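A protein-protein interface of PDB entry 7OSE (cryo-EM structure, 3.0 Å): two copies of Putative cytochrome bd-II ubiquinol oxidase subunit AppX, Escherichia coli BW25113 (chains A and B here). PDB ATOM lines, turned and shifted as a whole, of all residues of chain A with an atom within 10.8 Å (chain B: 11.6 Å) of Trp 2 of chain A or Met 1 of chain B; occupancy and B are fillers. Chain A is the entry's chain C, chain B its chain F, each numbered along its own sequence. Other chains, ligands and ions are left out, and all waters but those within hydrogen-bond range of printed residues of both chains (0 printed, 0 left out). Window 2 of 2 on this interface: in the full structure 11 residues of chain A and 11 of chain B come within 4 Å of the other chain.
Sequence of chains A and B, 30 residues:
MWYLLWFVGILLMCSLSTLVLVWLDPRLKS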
ATOM      1  N   MET A   1      21.594  20.509  29.461  1.00  0.00           N
ATOM      2  CA  MET A   1      21.245  20.283  28.065  1.00  0.00           C
ATOM      3  C   MET A   1      20.193  21.290  27.614  1.00  0.00           C
ATOM      4  O   MET A   1      19.737  21.261  26.472  1.00  0.00           O
ATOM      5  CB  MET A   1      20.741  18.852  27.864  1.00  0.00           C
ATOM      6  CG  MET A   1      20.872  18.331  26.442  1.00  0.00           C
ATOM      7  SD  MET A   1      20.388  16.604  26.288  1.00  0.00           S
ATOM      8  CE  MET A   1      18.669  16.693  26.778  1.00  0.00           C
ATOM      9  N   TRP A   2      19.814  22.191  28.523  1.00  0.00           N
ATOM     10  CA  TRP A   2      18.812  23.200  28.199  1.00  0.00           C
ATOM     11  C   TRP A   2      19.313  24.222  27.188  1.00  0.00           C
ATOM     12  O   TRP A   2      18.496  24.931  26.597  1.00  0.00           O
ATOM     13  CB  TRP A   2      18.355  23.924  29.463  1.00  0.00           C
ATOM     14  CG  TRP A   2      17.285  23.212  30.219  1.00  0.00           C
ATOM     15  CD1 TRP A   2      17.442  22.441  31.333  1.00  0.00           C
ATOM     16  CD2 TRP A   2      15.885  23.209  29.923  1.00  0.00           C
ATOM     17  NE1 TRP A   2      16.226  21.956  31.747  1.00  0.00           N
ATOM     18  CE2 TRP A   2      15.254  22.413  30.898  1.00  0.00           C
ATOM     19  CE3 TRP A   2      15.105  23.801  28.928  1.00  0.00           C
ATOM     20  CZ2 TRP A   2      13.881  22.194  30.905  1.00  0.00           C
ATOM     21  CZ3 TRP A   2      13.741  23.581  28.936  1.00  0.00           C
ATOM     22  CH2 TRP A   2      13.143  22.785  29.917  1.00  0.00           C
ATOM     23  N   TYR A   3      20.626  24.328  26.984  1.00  0.00           N
ATOM     24  CA  TYR A   3      21.141  25.294  26.016  1.00  0.00           C
ATOM     25  C   TYR A   3      20.775  24.890  24.593  1.00  0.00           C
ATOM     26  O   TYR A   3      20.264  25.704  23.813  1.00  0.00           O
ATOM     27  CB  TYR A   3      22.655  25.431  26.167  1.00  0.00           C
ATOM     28  CG  TYR A   3      23.106  25.848  27.549  1.00  0.00           C
ATOM     29  CD1 TYR A   3      22.267  26.563  28.390  1.00  0.00           C
ATOM     30  CD2 TYR A   3      24.374  25.526  28.011  1.00  0.00           C
ATOM     31  CE1 TYR A   3      22.675  26.942  29.651  1.00  0.00           C
ATOM     32  CE2 TYR A   3      24.792  25.903  29.270  1.00  0.00           C
ATOM     33  CZ  TYR A   3      23.939  26.611  30.086  1.00  0.00           C
ATOM     34  OH  TYR A   3      24.349  26.989  31.342  1.00  0.00           O
ATOM     35  N   LEU A   4      21.022  23.626  24.240  1.00  0.00           N
ATOM     36  CA  LEU A   4      20.639  23.137  22.921  1.00  0.00           C
ATOM     37  C   LEU A   4      19.128  23.160  22.752  1.00  0.00           C
ATOM     38  O   LEU A   4      18.617  23.476  21.669  1.00  0.00           O
ATOM     39  CB  LEU A   4      21.183  21.727  22.707  1.00  0.00           C
ATOM     40  CG  LEU A   4      20.991  21.137  21.311  1.00  0.00           C
ATOM     41  CD1 LEU A   4      21.626  22.037  20.266  1.00  0.00           C
ATOM     42  CD2 LEU A   4      21.576  19.739  21.241  1.00  0.00           C
ATOM     43  N   LEU A   5      18.395  22.821  23.814  1.00  0.00           N
ATOM     44  CA  LEU A   5      16.940  22.881  23.757  1.00  0.00           C
ATOM     45  C   LEU A   5      16.467  24.301  23.483  1.00  0.00           C
ATOM     46  O   LEU A   5      15.565  24.512  22.669  1.00  0.00           O
ATOM     47  CB  LEU A   5      16.344  22.351  25.062  1.00  0.00           C
ATOM     48  CG  LEU A   5      14.921  21.789  25.034  1.00  0.00           C
ATOM     49  CD1 LEU A   5      14.704  20.867  26.222  1.00  0.00           C
ATOM     50  CD2 LEU A   5      13.879  22.895  25.030  1.00  0.00           C
ATOM     51  N   TRP A   6      17.074  25.290  24.144  1.00  0.00           N
ATOM     52  CA  TRP A   6      16.707  26.679  23.895  1.00  0.00           C
ATOM     53  C   TRP A   6      17.039  27.093  22.471  1.00  0.00           C
ATOM     54  O   TRP A   6      16.268  27.817  21.835  1.00  0.00           O
ATOM     55  CB  TRP A   6      17.413  27.607  24.880  1.00  0.00           C
ATOM     56  CG  TRP A   6      17.472  29.016  24.375  1.00  0.00           C
ATOM     57  CD1 TRP A   6      16.509  29.971  24.501  1.00  0.00           C
ATOM     58  CD2 TRP A   6      18.545  29.621  23.641  1.00  0.00           C
ATOM     59  NE1 TRP A   6      16.916  31.135  23.899  1.00  0.00           N
ATOM     60  CE2 TRP A   6      18.163  30.946  23.363  1.00  0.00           C
ATOM     61  CE3 TRP A   6      19.790  29.171  23.196  1.00  0.00           C
ATOM     62  CZ2 TRP A   6      18.981  31.825  22.662  1.00  0.00           C
ATOM     63  CZ3 TRP A   6      20.601  30.045  22.500  1.00  0.00           C
ATOM     64  CH2 TRP A   6      20.193  31.358  22.240  1.00  0.00           C
ATOM     65  N   PHE A   7      18.197  26.671  21.964  1.00  0.00           N
ATOM     66  CA  PHE A   7      18.582  27.021  20.599  1.00  0.00           C
ATOM     67  C   PHE A   7      17.572  26.481  19.594  1.00  0.00           C
ATOM     68  O   PHE A   7      17.054  27.221  18.740  1.00  0.00           O
ATOM     69  CB  PHE A   7      19.983  26.478  20.317  1.00  0.00           C
ATOM     70  CG  PHE A   7      20.544  26.890  18.990  1.00  0.00           C
ATOM     71  CD1 PHE A   7      21.100  28.145  18.819  1.00  0.00           C
ATOM     72  CD2 PHE A   7      20.539  26.016  17.920  1.00  0.00           C
ATOM     73  CE1 PHE A   7      21.625  28.524  17.600  1.00  0.00           C
ATOM     74  CE2 PHE A   7      21.064  26.389  16.700  1.00  0.00           C
ATOM     75  CZ  PHE A   7      21.607  27.645  16.540  1.00  0.00           C
ATOM     76  N   VAL A   8      17.257  25.190  19.703  1.00  0.00           N
ATOM     77  CA  VAL A   8      16.287  24.583  18.799  1.00  0.00           C
ATOM     78  C   VAL A   8      14.920  25.235  18.972  1.00  0.00           C
ATOM     79  O   VAL A   8      14.207  25.476  17.994  1.00  0.00           O
ATOM     80  CB  VAL A   8      16.229  23.061  19.023  1.00  0.00           C
ATOM     81  CG1 VAL A   8      15.228  22.424  18.086  1.00  0.00           C
ATOM     82  CG2 VAL A   8      17.603  22.447  18.817  1.00  0.00           C
ATOM     83  N   GLY A   9      14.545  25.552  20.213  1.00  0.00           N
ATOM     84  CA  GLY A   9      13.243  26.147  20.457  1.00  0.00           C
ATOM     85  C   GLY A   9      13.103  27.543  19.884  1.00  0.00           C
ATOM     86  O   GLY A   9      12.056  27.891  19.334  1.00  0.00           O
ATOM     87  N   ILE A  10      14.142  28.369  20.011  1.00  0.00           N
ATOM     88  CA  ILE A  10      14.058  29.720  19.470  1.00  0.00           C
ATOM     89  C   ILE A  10      14.058  29.682  17.948  1.00  0.00           C
ATOM     90  O   ILE A  10      13.324  30.440  17.300  1.00  0.00           O
ATOM     91  CB  ILE A  10      15.178  30.621  20.029  1.00  0.00           C
ATOM     92  CG1 ILE A  10      15.003  32.053  19.524  1.00  0.00           C
ATOM     93  CG2 ILE A  10      16.549  30.117  19.638  1.00  0.00           C
ATOM     94  CD1 ILE A  10      13.618  32.617  19.739  1.00  0.00           C
ATOM     95  N   LEU A  11      14.851  28.789  17.347  1.00  0.00           N
ATOM     96  CA  LEU A  11      14.777  28.650  15.896  1.00  0.00           C
ATOM     97  C   LEU A  11      13.396  28.168  15.462  1.00  0.00           C
ATOM     98  O   LEU A  11      12.858  28.625  14.445  1.00  0.00           O
ATOM     99  CB  LEU A  11      15.866  27.706  15.395  1.00  0.00           C
ATOM    100  CG  LEU A  11      17.280  28.279  15.346  1.00  0.00           C
ATOM    101  CD1 LEU A  11      18.233  27.283  14.710  1.00  0.00           C
ATOM    102  CD2 LEU A  11      17.290  29.592  14.586  1.00  0.00           C
ATOM    103  N   MET B   1      15.115  13.793  28.889  1.00  0.00           N
ATOM    104  CA  MET B   1      14.583  15.042  28.359  1.00  0.00           C
ATOM    105  C   MET B   1      14.737  15.080  26.843  1.00  0.00           C
ATOM    106  O   MET B   1      14.374  16.060  26.194  1.00  0.00           O
ATOM    107  CB  MET B   1      15.290  16.238  29.001  1.00  0.00           C
ATOM    108  CG  MET B   1      14.493  17.532  28.966  1.00  0.00           C
ATOM    109  SD  MET B   1      15.309  18.874  29.847  1.00  0.00           S
ATOM    110  CE  MET B   1      16.818  19.029  28.897  1.00  0.00           C
ATOM    111  N   TRP B   2      15.273  13.996  26.279  1.00  0.00           N
ATOM    112  CA  TRP B   2      15.467  13.926  24.835  1.00  0.00           C
ATOM    113  C   TRP B   2      14.154  13.846  24.068  1.00  0.00           C
ATOM    114  O   TRP B   2      14.149  14.092  22.860  1.00  0.00           O
ATOM    115  CB  TRP B   2      16.334  12.723  24.471  1.00  0.00           C
ATOM    116  CG  TRP B   2      17.801  12.975  24.580  1.00  0.00           C
ATOM    117  CD1 TRP B   2      18.621  12.610  25.606  1.00  0.00           C
ATOM    118  CD2 TRP B   2      18.628  13.643  23.623  1.00  0.00           C
ATOM    119  NE1 TRP B   2      19.908  13.012  25.348  1.00  0.00           N
ATOM    120  CE2 TRP B   2      19.938  13.649  24.136  1.00  0.00           C
ATOM    121  CE3 TRP B   2      18.386  14.239  22.383  1.00  0.00           C
ATOM    122  CZ2 TRP B   2      21.003  14.227  23.452  1.00  0.00           C
ATOM    123  CZ3 TRP B   2      19.444  14.813  21.706  1.00  0.00           C
ATOM    124  CH2 TRP B   2      20.735  14.803  22.241  1.00  0.00           C
ATOM    125  N   TYR B   3      13.049  13.499  24.728  1.00  0.00           N
ATOM    126  CA  TYR B   3      11.770  13.421  24.025  1.00  0.00           C
ATOM    127  C   TYR B   3      11.293  14.804  23.603  1.00  0.00           C
ATOM    128  O   TYR B   3      10.918  15.020  22.444  1.00  0.00           O
ATOM    129  CB  TYR B   3      10.728  12.735  24.908  1.00  0.00           C
ATOM    130  CG  TYR B   3      11.115  11.344  25.359  1.00  0.00           C
ATOM    131  CD1 TYR B   3      12.001  10.573  24.623  1.00  0.00           C
ATOM    132  CD2 TYR B   3      10.591  10.802  26.524  1.00  0.00           C
ATOM    133  CE1 TYR B   3      12.358   9.306  25.034  1.00  0.00           C
ATOM    134  CE2 TYR B   3      10.939   9.534  26.942  1.00  0.00           C
ATOM    135  CZ  TYR B   3      11.823   8.791  26.193  1.00  0.00           C
ATOM    136  OH  TYR B   3      12.173   7.528  26.604  1.00  0.00           O
ATOM    137  N   LEU B   4      11.310  15.761  24.535  1.00  0.00           N
ATOM    138  CA  LEU B   4      10.936  17.129  24.197  1.00  0.00           C
ATOM    139  C   LEU B   4      11.913  17.727  23.196  1.00  0.00           C
ATOM    140  O   LEU B   4      11.514  18.469  22.288  1.00  0.00           O
ATOM    141  CB  LEU B   4      10.873  17.981  25.463  1.00  0.00           C
ATOM    142  CG  LEU B   4      10.348  19.405  25.288  1.00  0.00           C
ATOM    143  CD1 LEU B   4       8.958  19.383  24.679  1.00  0.00           C
ATOM    144  CD2 LEU B   4      10.339  20.134  26.619  1.00  0.00           C
ATOM    145  N   LEU B   5      13.202  17.420  23.352  1.00  0.00           N
ATOM    146  CA  LEU B   5      14.195  17.896  22.398  1.00  0.00           C
ATOM    147  C   LEU B   5      13.905  17.363  21.003  1.00  0.00           C
ATOM    148  O   LEU B   5      13.987  18.105  20.021  1.00  0.00           O
ATOM    149  CB  LEU B   5      15.597  17.491  22.855  1.00  0.00           C
ATOM    150  CG  LEU B   5      16.788  18.323  22.373  1.00  0.00           C
ATOM    151  CD1 LEU B   5      17.972  18.121  23.302  1.00  0.00           C
ATOM    152  CD2 LEU B   5      17.174  17.977  20.945  1.00  0.00           C
ATOM    153  N   TRP B   6      13.551  16.080  20.895  1.00  0.00           N
ATOM    154  CA  TRP B   6      13.211  15.513  19.596  1.00  0.00           C
ATOM    155  C   TRP B   6      11.964  16.162  19.018  1.00  0.00           C
ATOM    156  O   TRP B   6      11.893  16.416  17.813  1.00  0.00           O
ATOM    157  CB  TRP B   6      13.005  14.004  19.704  1.00  0.00           C
ATOM    158  CG  TRP B   6      12.193  13.469  18.565  1.00  0.00           C
ATOM    159  CD1 TRP B   6      12.652  13.100  17.337  1.00  0.00           C
ATOM    160  CD2 TRP B   6      10.775  13.267  18.541  1.00  0.00           C
ATOM    161  NE1 TRP B   6      11.611  12.672  16.551  1.00  0.00           N
ATOM    162  CE2 TRP B   6      10.447  12.766  17.267  1.00  0.00           C
ATOM    163  CE3 TRP B   6       9.752  13.458  19.473  1.00  0.00           C
ATOM    164  CZ2 TRP B   6       9.142  12.452  16.903  1.00  0.00           C
ATOM    165  CZ3 TRP B   6       8.457  13.147  19.109  1.00  0.00           C
ATOM    166  CH2 TRP B   6       8.164  12.648  17.836  1.00  0.00           C
ATOM    167  N   PHE B   7      10.957  16.408  19.857  1.00  0.00           N
ATOM    168  CA  PHE B   7       9.729  17.038  19.377  1.00  0.00           C
ATOM    169  C   PHE B   7      10.016  18.418  18.798  1.00  0.00           C
ATOM    170  O   PHE B   7       9.623  18.736  17.663  1.00  0.00           O
ATOM    171  CB  PHE B   7       8.724  17.121  20.526  1.00  0.00           C
ATOM    172  CG  PHE B   7       7.373  17.627  20.123  1.00  0.00           C
ATOM    173  CD1 PHE B   7       6.459  16.788  19.512  1.00  0.00           C
ATOM    174  CD2 PHE B   7       7.006  18.935  20.378  1.00  0.00           C
ATOM    175  CE1 PHE B   7       5.211  17.250  19.148  1.00  0.00           C
ATOM    176  CE2 PHE B   7       5.759  19.401  20.017  1.00  0.00           C
ATOM    177  CZ  PHE B   7       4.861  18.558  19.400  1.00  0.00           C
ATOM    178  N   VAL B   8      10.730  19.246  19.562  1.00  0.00           N
ATOM    179  CA  VAL B   8      11.072  20.584  19.091  1.00  0.00           C
ATOM    180  C   VAL B   8      11.949  20.500  17.848  1.00  0.00           C
ATOM    181  O   VAL B   8      11.785  21.279  16.904  1.00  0.00           O
ATOM    182  CB  VAL B   8      11.747  21.389  20.217  1.00  0.00           C
ATOM    183  CG1 VAL B   8      12.100  22.778  19.737  1.00  0.00           C
ATOM    184  CG2 VAL B   8      10.831  21.471  21.426  1.00  0.00           C
ATOM    185  N   GLY B   9      12.876  19.540  17.816  1.00  0.00           N
ATOM    186  CA  GLY B   9      13.769  19.420  16.678  1.00  0.00           C
ATOM    187  C   GLY B   9      13.064  19.006  15.400  1.00  0.00           C
ATOM    188  O   GLY B   9      13.368  19.522  14.323  1.00  0.00           O
ATOM    189  N   ILE B  10      12.126  18.064  15.492  1.00  0.00           N
ATOM    190  CA  ILE B  10      11.415  17.637  14.294  1.00  0.00           C
ATOM    191  C   ILE B  10      10.494  18.745  13.801  1.00  0.00           C
ATOM    192  O   ILE B  10      10.378  18.974  12.591  1.00  0.00           O
ATOM    193  CB  ILE B  10      10.657  16.315  14.531  1.00  0.00           C
ATOM    194  CG1 ILE B  10      10.008  15.840  13.231  1.00  0.00           C
ATOM    195  CG2 ILE B  10       9.595  16.460  15.596  1.00  0.00           C
ATOM    196  CD1 ILE B  10      10.952  15.788  12.053  1.00  0.00           C
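The indole nitrogen (NE1) of Trp 2 of chain A lies close to the side-chain sulfur (SD) of Met 1 of chain B (3.7 Å). The side-chain sulfur (SD) of Met 1 of chain A lies close to the indole nitrogen (NE1) of Trp 2 of chain B (3.7 Å).
Among the printed residues, pairs that only touch across the chains: Met 1 of chain A with Met 1 of chain B, Met 1 of chain A with Leu 5 of chain B, Leu 5 of chain A with Met 1 of chain B, Val 8 of chain A with Val 8 of chain B, Val 8 of chain A with Gly 9 of chain B and Gly 9 of chain A with Val 8 of chain B.
Met 1 of chain A touches just these residues of chain B: Met 1 (3.7 Å), Trp 2 (3.7 Å) and Leu 5 (3.8 Å). Trp 2 of chain A touches one residue of chain B. No residue of chain B comes within 4 Å of Tyr 3 of chain A. Printed residues of chain B within 4 Å of Val 8 of chain A: Val 8 (3.6 Å) and Gly 9 (3.6 Å). Printed residues of chain B within 4 Å of Gly 9 of chain A: Val 8 (3.6 Å). No residue of chain A comes within 4 Å of Leu 4 of chain B. Trp 6 of chain B touches none of the printed residues of chain A. Of the printed residues of chain A, Gly 9 of chain B touches Val 8 (3.6 Å). The nearest residue of chain B that does not touch Trp 2 of chain A is Leu 4 of chain B (5.1 Å). The nearest residue of chain A that does not touch Met 1 of chain B is Tyr 3 of chain A (6.8 Å).
Hydrophobic or aromatic side chains of chain B that line the printed part of chain A: Met 1, Trp 2, Leu 5 and Val 8. Of the 11 printed residues of chain A, 5 touch a printed residue of chain B. Printed residues of chain A that touch a printed residue of chain B: Met 1, Trp 2, Leu 5, Val 8 and Gly 9. Among the printed residues, 8 pairs touch across the chains. Among the printed residues, no Asp or Glu carboxylate lies within 4 Å of a Lys or Arg side-chain nitrogen of the other chain.
Met 1 of chain A touches its own counterpart, Met 1 of chain B. Met 1 of chain A touches Trp 2 of chain B, and with the chains exchanged Trp 2 of chain A touches Met 1 of chain B. Met 1 of chain A touches Leu 5 of chain B, and with the chains exchanged Leu 5 of chain A touches Met 1 of chain B. Val 8 of chain A touches its own counterpart, Val 8 of chain B. 10 positions are printed for both chains. Of the 8 pairs that touch across the chains among the printed residues, 8 have their exchanged pair printed and touching as well.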
